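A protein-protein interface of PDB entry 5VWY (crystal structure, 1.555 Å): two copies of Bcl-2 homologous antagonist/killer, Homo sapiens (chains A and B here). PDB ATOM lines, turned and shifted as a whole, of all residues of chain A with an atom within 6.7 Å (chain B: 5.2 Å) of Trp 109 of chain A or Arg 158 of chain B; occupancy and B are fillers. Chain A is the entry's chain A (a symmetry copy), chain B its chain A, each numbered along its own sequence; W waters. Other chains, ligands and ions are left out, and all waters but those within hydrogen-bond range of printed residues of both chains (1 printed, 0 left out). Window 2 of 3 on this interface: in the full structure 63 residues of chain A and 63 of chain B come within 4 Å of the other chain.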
ATOM      1  N   VAL A  58     -37.480  20.274  -9.696  1.00  0.00           N
ATOM      2  CA  VAL A  58     -36.518  19.727 -10.649  1.00  0.00           C
ATOM      3  C   VAL A  58     -36.619  18.210 -10.684  1.00  0.00           C
ATOM      4  O   VAL A  58     -36.740  17.597 -11.751  1.00  0.00           O
ATOM      5  CB  VAL A  58     -35.093  20.196 -10.307  1.00  0.00           C
ATOM      6  CG1 VAL A  58     -34.060  19.405 -11.125  1.00  0.00           C
ATOM      7  CG2 VAL A  58     -34.959  21.707 -10.538  1.00  0.00           C
ATOM      8  N   LEU A  62     -37.905  15.948 -14.018  1.00  0.00           N
ATOM      9  CA  LEU A  62     -37.034  14.993 -14.693  1.00  0.00           C
ATOM     10  C   LEU A  62     -37.631  13.599 -14.673  1.00  0.00           C
ATOM     11  O   LEU A  62     -37.438  12.827 -15.623  1.00  0.00           O
ATOM     12  CB  LEU A  62     -35.633  14.982 -14.071  1.00  0.00           C
ATOM     13  CG  LEU A  62     -34.893  16.320 -14.138  1.00  0.00           C
ATOM     14  CD1 LEU A  62     -33.586  16.318 -13.333  1.00  0.00           C
ATOM     15  CD2 LEU A  62     -34.626  16.763 -15.580  1.00  0.00           C
ATOM     16  N   ILE A 107     -19.955  14.240 -19.744  1.00  0.00           N
ATOM     17  CA  ILE A 107     -21.146  14.548 -18.960  1.00  0.00           C
ATOM     18  C   ILE A 107     -22.106  15.319 -19.851  1.00  0.00           C
ATOM     19  O   ILE A 107     -21.699  16.257 -20.549  1.00  0.00           O
ATOM     20  CB  ILE A 107     -20.810  15.387 -17.718  1.00  0.00           C
ATOM     21  CG1 ILE A 107     -19.676  14.749 -16.896  1.00  0.00           C
ATOM     22  CG2 ILE A 107     -22.062  15.622 -16.889  1.00  0.00           C
ATOM     23  CD1 ILE A 107     -19.209  15.649 -15.769  1.00  0.00           C
ATOM     24  N   ASN A 108     -23.374  14.933 -19.831  1.00  0.00           N
ATOM     25  CA  ASN A 108     -24.417  15.789 -20.365  1.00  0.00           C
ATOM     26  C   ASN A 108     -25.626  15.631 -19.464  1.00  0.00           C
ATOM     27  O   ASN A 108     -25.623  14.799 -18.551  1.00  0.00           O
ATOM     28  CB  ASN A 108     -24.710  15.487 -21.851  1.00  0.00           C
ATOM     29  CG  ASN A 108     -25.240  14.083 -22.086  1.00  0.00           C
ATOM     30  OD1 ASN A 108     -26.138  13.633 -21.373  1.00  0.00           O
ATOM     31  ND2 ASN A 108     -24.716  13.392 -23.112  1.00  0.00           N
ATOM     32  N   TRP A 109     -26.646  16.471 -19.678  1.00  0.00           N
ATOM     33  CA  TRP A 109     -27.802  16.432 -18.780  1.00  0.00           C
ATOM     34  C   TRP A 109     -28.461  15.061 -18.772  1.00  0.00           C
ATOM     35  O   TRP A 109     -28.857  14.562 -17.705  1.00  0.00           O
ATOM     36  CB  TRP A 109     -28.825  17.502 -19.161  1.00  0.00           C
ATOM     37  CG  TRP A 109     -28.548  18.851 -18.617  1.00  0.00           C
ATOM     38  CD1 TRP A 109     -28.275  19.987 -19.338  1.00  0.00           C
ATOM     39  CD2 TRP A 109     -28.532  19.240 -17.237  1.00  0.00           C
ATOM     40  NE1 TRP A 109     -28.093  21.056 -18.486  1.00  0.00           N
ATOM     41  CE2 TRP A 109     -28.242  20.622 -17.195  1.00  0.00           C
ATOM     42  CE3 TRP A 109     -28.727  18.548 -16.030  1.00  0.00           C
ATOM     43  CZ2 TRP A 109     -28.147  21.331 -16.001  1.00  0.00           C
ATOM     44  CZ3 TRP A 109     -28.643  19.260 -14.836  1.00  0.00           C
ATOM     45  CH2 TRP A 109     -28.344  20.635 -14.835  1.00  0.00           C
ATOM     46  N   GLY A 110     -28.585  14.434 -19.948  1.00  0.00           N
ATOM     47  CA  GLY A 110     -29.233  13.137 -20.023  1.00  0.00           C
ATOM     48  C   GLY A 110     -28.508  12.078 -19.216  1.00  0.00           C
ATOM     49  O   GLY A 110     -29.137  11.259 -18.550  1.00  0.00           O
ATOM     50  N   ARG A 111     -27.174  12.095 -19.242  1.00  0.00           N
ATOM     51  CA  ARG A 111     -26.432  11.128 -18.435  1.00  0.00           C
ATOM     52  C   ARG A 111     -26.565  11.423 -16.950  1.00  0.00           C
ATOM     53  O   ARG A 111     -26.568  10.493 -16.123  1.00  0.00           O
ATOM     54  CB  ARG A 111     -24.962  11.119 -18.846  1.00  0.00           C
ATOM     55  CG  ARG A 111     -24.757  10.556 -20.241  1.00  0.00           C
ATOM     56  CD  ARG A 111     -23.310  10.701 -20.705  1.00  0.00           C
ATOM     57  NE  ARG A 111     -23.208  10.309 -22.109  1.00  0.00           N
ATOM     58  CZ  ARG A 111     -22.064  10.119 -22.744  1.00  0.00           C
ATOM     59  NH1 ARG A 111     -20.926  10.292 -22.095  1.00  0.00           N
ATOM     60  NH2 ARG A 111     -22.047   9.739 -24.021  1.00  0.00           N
ATOM     61  N   VAL A 112     -26.683  12.703 -16.581  1.00  0.00           N
ATOM     62  CA  VAL A 112     -26.945  13.042 -15.183  1.00  0.00           C
ATOM     63  C   VAL A 112     -28.291  12.467 -14.755  1.00  0.00           C
ATOM     64  O   VAL A 112     -28.406  11.865 -13.682  1.00  0.00           O
ATOM     65  CB  VAL A 112     -26.885  14.563 -14.966  1.00  0.00           C
ATOM     66  CG1 VAL A 112     -27.357  14.929 -13.535  1.00  0.00           C
ATOM     67  CG2 VAL A 112     -25.470  15.065 -15.178  1.00  0.00           C
ATOM     68  N   VAL A 113     -29.318  12.597 -15.609  1.00  0.00           N
ATOM     69  CA  VAL A 113     -30.625  12.028 -15.278  1.00  0.00           C
ATOM     70  C   VAL A 113     -30.542  10.506 -15.215  1.00  0.00           C
ATOM     71  O   VAL A 113     -31.196   9.873 -14.367  1.00  0.00           O
ATOM     72  CB  VAL A 113     -31.707  12.507 -16.271  1.00  0.00           C
ATOM     73  CG1 VAL A 113     -33.066  11.899 -15.920  1.00  0.00           C
ATOM     74  CG2 VAL A 113     -31.821  14.026 -16.239  1.00  0.00           C
ATOM     75  N   ALA A 114     -29.726   9.896 -16.081  1.00  0.00           N
ATOM     76  CA  ALA A 114     -29.558   8.446 -16.055  1.00  0.00           C
ATOM     77  C   ALA A 114     -28.953   7.994 -14.733  1.00  0.00           C
ATOM     78  O   ALA A 114     -29.269   6.897 -14.249  1.00  0.00           O
ATOM     79  CB  ALA A 114     -28.695   7.981 -17.232  1.00  0.00           C
ATOM     80  N   TRP B 154     -19.814  20.106 -12.907  1.00  0.00           N
ATOM     81  CA  TRP B 154     -20.405  20.311 -14.225  1.00  0.00           C
ATOM     82  C   TRP B 154     -21.768  20.977 -14.115  1.00  0.00           C
ATOM     83  O   TRP B 154     -22.064  21.948 -14.825  1.00  0.00           O
ATOM     84  CB  TRP B 154     -20.508  18.971 -14.951  1.00  0.00           C
ATOM     85  CG  TRP B 154     -21.026  19.077 -16.332  1.00  0.00           C
ATOM     86  CD1 TRP B 154     -20.290  19.267 -17.458  1.00  0.00           C
ATOM     87  CD2 TRP B 154     -22.398  19.024 -16.745  1.00  0.00           C
ATOM     88  NE1 TRP B 154     -21.113  19.309 -18.562  1.00  0.00           N
ATOM     89  CE2 TRP B 154     -22.412  19.191 -18.149  1.00  0.00           C
ATOM     90  CE3 TRP B 154     -23.613  18.869 -16.069  1.00  0.00           C
ATOM     91  CZ2 TRP B 154     -23.594  19.164 -18.892  1.00  0.00           C
ATOM     92  CZ3 TRP B 154     -24.786  18.847 -16.803  1.00  0.00           C
ATOM     93  CH2 TRP B 154     -24.765  19.008 -18.200  1.00  0.00           C
ATOM     94  N   ILE B 155     -22.611  20.470 -13.221  1.00  0.00           N
ATOM     95  CA  ILE B 155     -23.934  21.054 -13.045  1.00  0.00           C
ATOM     96  C   ILE B 155     -23.821  22.508 -12.615  1.00  0.00           C
ATOM     97  O   ILE B 155     -24.568  23.371 -13.093  1.00  0.00           O
ATOM     98  CB  ILE B 155     -24.741  20.214 -12.040  1.00  0.00           C
ATOM     99  CG1 ILE B 155     -25.034  18.841 -12.644  1.00  0.00           C
ATOM    100  CG2 ILE B 155     -26.030  20.915 -11.670  1.00  0.00           C
ATOM    101  CD1 ILE B 155     -25.701  17.928 -11.630  1.00  0.00           C
ATOM    102  N   ALA B 156     -22.883  22.812 -11.712  1.00  0.00           N
ATOM    103  CA  ALA B 156     -22.689  24.196 -11.295  1.00  0.00           C
ATOM    104  C   ALA B 156     -22.359  25.087 -12.487  1.00  0.00           C
ATOM    105  O   ALA B 156     -22.933  26.167 -12.635  1.00  0.00           O
ATOM    106  CB  ALA B 156     -21.589  24.278 -10.241  1.00  0.00           C
ATOM    107  N   GLN B 157     -21.499  24.615 -13.386  1.00  0.00           N
ATOM    108  CA  GLN B 157     -21.120  25.449 -14.522  1.00  0.00           C
ATOM    109  C   GLN B 157     -22.231  25.572 -15.554  1.00  0.00           C
ATOM    110  O   GLN B 157     -22.224  26.534 -16.334  1.00  0.00           O
ATOM    111  CB  GLN B 157     -19.846  24.912 -15.159  1.00  0.00           C
ATOM    112  CG  GLN B 157     -18.632  25.189 -14.307  1.00  0.00           C
ATOM    113  CD  GLN B 157     -17.376  24.623 -14.895  1.00  0.00           C
ATOM    114  OE1 GLN B 157     -17.401  24.029 -15.967  1.00  0.00           O
ATOM    115  NE2 GLN B 157     -16.263  24.799 -14.195  1.00  0.00           N
ATOM    116  N   ARG B 158     -23.191  24.649 -15.563  1.00  0.00           N
ATOM    117  CA  ARG B 158     -24.364  24.777 -16.420  1.00  0.00           C
ATOM    118  C   ARG B 158     -25.468  25.612 -15.780  1.00  0.00           C
ATOM    119  O   ARG B 158     -26.557  25.706 -16.357  1.00  0.00           O
ATOM    120  CB  ARG B 158     -24.930  23.402 -16.793  1.00  0.00           C
ATOM    121  CG  ARG B 158     -23.994  22.517 -17.601  1.00  0.00           C
ATOM    122  CD  ARG B 158     -23.480  23.203 -18.847  1.00  0.00           C
ATOM    123  NE  ARG B 158     -24.537  23.668 -19.747  1.00  0.00           N
ATOM    124  CZ  ARG B 158     -25.176  22.891 -20.618  1.00  0.00           C
ATOM    125  NH1 ARG B 158     -24.878  21.603 -20.716  1.00  0.00           N
ATOM    126  NH2 ARG B 158     -26.115  23.404 -21.397  1.00  0.00           N
ATOM    127  N   GLY B 159     -25.229  26.180 -14.600  1.00  0.00           N
ATOM    128  CA  GLY B 159     -26.217  26.989 -13.909  1.00  0.00           C
ATOM    129  C   GLY B 159     -26.910  26.344 -12.723  1.00  0.00           C
ATOM    130  O   GLY B 159     -27.908  26.895 -12.242  1.00  0.00           O
ATOM    131  N   GLY B 160     -26.418  25.205 -12.229  1.00  0.00           N
ATOM    132  CA  GLY B 160     -27.054  24.548 -11.100  1.00  0.00           C
ATOM    133  C   GLY B 160     -28.212  23.664 -11.530  1.00  0.00           C
ATOM    134  O   GLY B 160     -28.600  23.594 -12.696  1.00  0.00           O
ATOM    135  N   TRP B 161     -28.774  22.958 -10.548  1.00  0.00           N
ATOM    136  CA  TRP B 161     -29.889  22.064 -10.845  1.00  0.00           C
ATOM    137  C   TRP B 161     -31.080  22.819 -11.414  1.00  0.00           C
ATOM    138  O   TRP B 161     -31.833  22.265 -12.224  1.00  0.00           O
ATOM    139  CB  TRP B 161     -30.307  21.309  -9.586  1.00  0.00           C
ATOM    140  CG  TRP B 161     -29.534  20.063  -9.310  1.00  0.00           C
ATOM    141  CD1 TRP B 161     -28.666  19.861  -8.267  1.00  0.00           C
ATOM    142  CD2 TRP B 161     -29.587  18.829 -10.040  1.00  0.00           C
ATOM    143  NE1 TRP B 161     -28.154  18.582  -8.326  1.00  0.00           N
ATOM    144  CE2 TRP B 161     -28.712  17.922  -9.390  1.00  0.00           C
ATOM    145  CE3 TRP B 161     -30.300  18.393 -11.162  1.00  0.00           C
ATOM    146  CZ2 TRP B 161     -28.527  16.603  -9.828  1.00  0.00           C
ATOM    147  CZ3 TRP B 161     -30.109  17.071 -11.600  1.00  0.00           C
ATOM    148  CH2 TRP B 161     -29.228  16.201 -10.934  1.00  0.00           C
ATOM    149  N   ALA B 163     -31.211  24.914 -13.590  1.00  0.00           N
ATOM    150  CA  ALA B 163     -31.152  25.005 -15.052  1.00  0.00           C
ATOM    151  C   ALA B 163     -31.806  23.811 -15.733  1.00  0.00           C
ATOM    152  O   ALA B 163     -32.219  23.921 -16.894  1.00  0.00           O
ATOM    153  CB  ALA B 163     -29.703  25.137 -15.519  1.00  0.00           C
ATOM    154  N   ALA B 164     -31.924  22.678 -15.044  1.00  0.00           N
ATOM    155  CA  ALA B 164     -32.634  21.541 -15.617  1.00  0.00           C
ATOM    156  C   ALA B 164     -34.119  21.828 -15.831  1.00  0.00           C
ATOM    157  O   ALA B 164     -34.799  21.043 -16.495  1.00  0.00           O
ATOM    158  CB  ALA B 164     -32.445  20.307 -14.721  1.00  0.00           C
ATOM    159  N   LEU B 167     -35.364  21.677 -19.426  1.00  0.00           N
ATOM    160  CA  LEU B 167     -35.521  20.421 -20.150  1.00  0.00           C
ATOM    161  C   LEU B 167     -37.003  20.065 -20.232  1.00  0.00           C
ATOM    162  O   LEU B 167     -37.676  19.943 -19.201  1.00  0.00           O
ATOM    163  CB  LEU B 167     -34.726  19.322 -19.448  1.00  0.00           C
ATOM    164  CG  LEU B 167     -33.228  19.631 -19.315  1.00  0.00           C
ATOM    165  CD1 LEU B 167     -32.567  18.732 -18.245  1.00  0.00           C
ATOM    166  CD2 LEU B 167     -32.536  19.451 -20.652  1.00  0.00           C
HETATM  167  O   HOH W   1     -28.176  23.871 -18.900  1.00  0.00           O
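The backbone NH of Gly 110 of chain A sits at hydrogen-bond distance from the side-chain amide oxygen of Asn 108 of chain A (2.9 Å).
The backbone carbonyl oxygen (O) of Ile 155 of chain B is in hydrogen-bond range of the backbone NH (N) of Gly 160 of chain B (2.7 Å).
OD1 of Asn 108 of chain A is in hydrogen-bond range of N of Arg 111 of chain A.
O of Trp 161 of chain B touches CG2 of Val 58 of chain A, at 3.6 Å.
Leu 62 of chain A touches Leu 167 of chain B.
Trp 154 of chain B touches Ile 107 of chain A (CD2 to CG2, 3.4 Å).
Asn 108 of chain A touches Trp 154 of chain B (C to CH2, 3.7 Å).
N of Trp 109 of chain A touches CH2 of Trp 154 of chain B (3.5 Å).
CZ2 of Trp 109 of chain A touches CB of Arg 158 of chain B, at 3.9 Å.
Gly 160 of chain B touches Trp 109 of chain A (O to CH2, 3.7 Å).
CZ3 of Trp 109 of chain A touches CB of Ala 164 of chain B (3.9 Å).
Val 112 of chain A touches Ile 155 of chain B.
Val 112 of chain A touches Trp 161 of chain B (CG1 to CH2, 3.4 Å).
Of the printed residues of chain B, Val 58 of chain A touches Trp 161.
Trp 109 of chain A touches just these residues of chain B: Trp 154 (3.5 Å), Ile 155 (3.9 Å), Arg 158 (3.9 Å), Gly 160 (3.7 Å) and Ala 164 (3.9 Å).
Of the printed residues of chain A, Trp 154 of chain B touches Ile 107, Asn 108 and Trp 109.
Of the printed residues of chain A, Ile 155 of chain B touches Trp 109 and Val 112.
Arg 158 of chain B touches just one residue of chain A: Trp 109.
Printed residues of chain A within 4 Å of Gly 160 of chain B: Trp 109 (3.7 Å).
Of the printed residues of chain A, Leu 167 of chain B touches Leu 62 (3.9 Å).
The nearest residue of chain A that does not touch Arg 158 of chain B is Asn 108 of chain A (5.8 Å).
The nearest printed residue of chain B that does not touch Leu 62 of chain A is Ala 164 of chain B (4.2 Å).
Hydrophobic or aromatic side chains of chain B that line the printed part of chain A: Trp 154, Ile 155, Trp 161, Ala 164 and Leu 167.
Printed residues of chain A that touch a printed residue of chain B: Val 58, Leu 62, Ile 107, Asn 108, Trp 109 and Val 112.
Among the printed residues, 12 pairs touch across the chains.
No position is printed for both chains.
Of the 12 pairs that touch across the chains among the printed residues, none has its exchanged pair printed and touching as well.
Water W1 lies within hydrogen-bond range of the indole nitrogen of Trp 109 of chain A (2.8 Å) and the guanidinium group of Arg 158 of chain B (3.3 Å).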
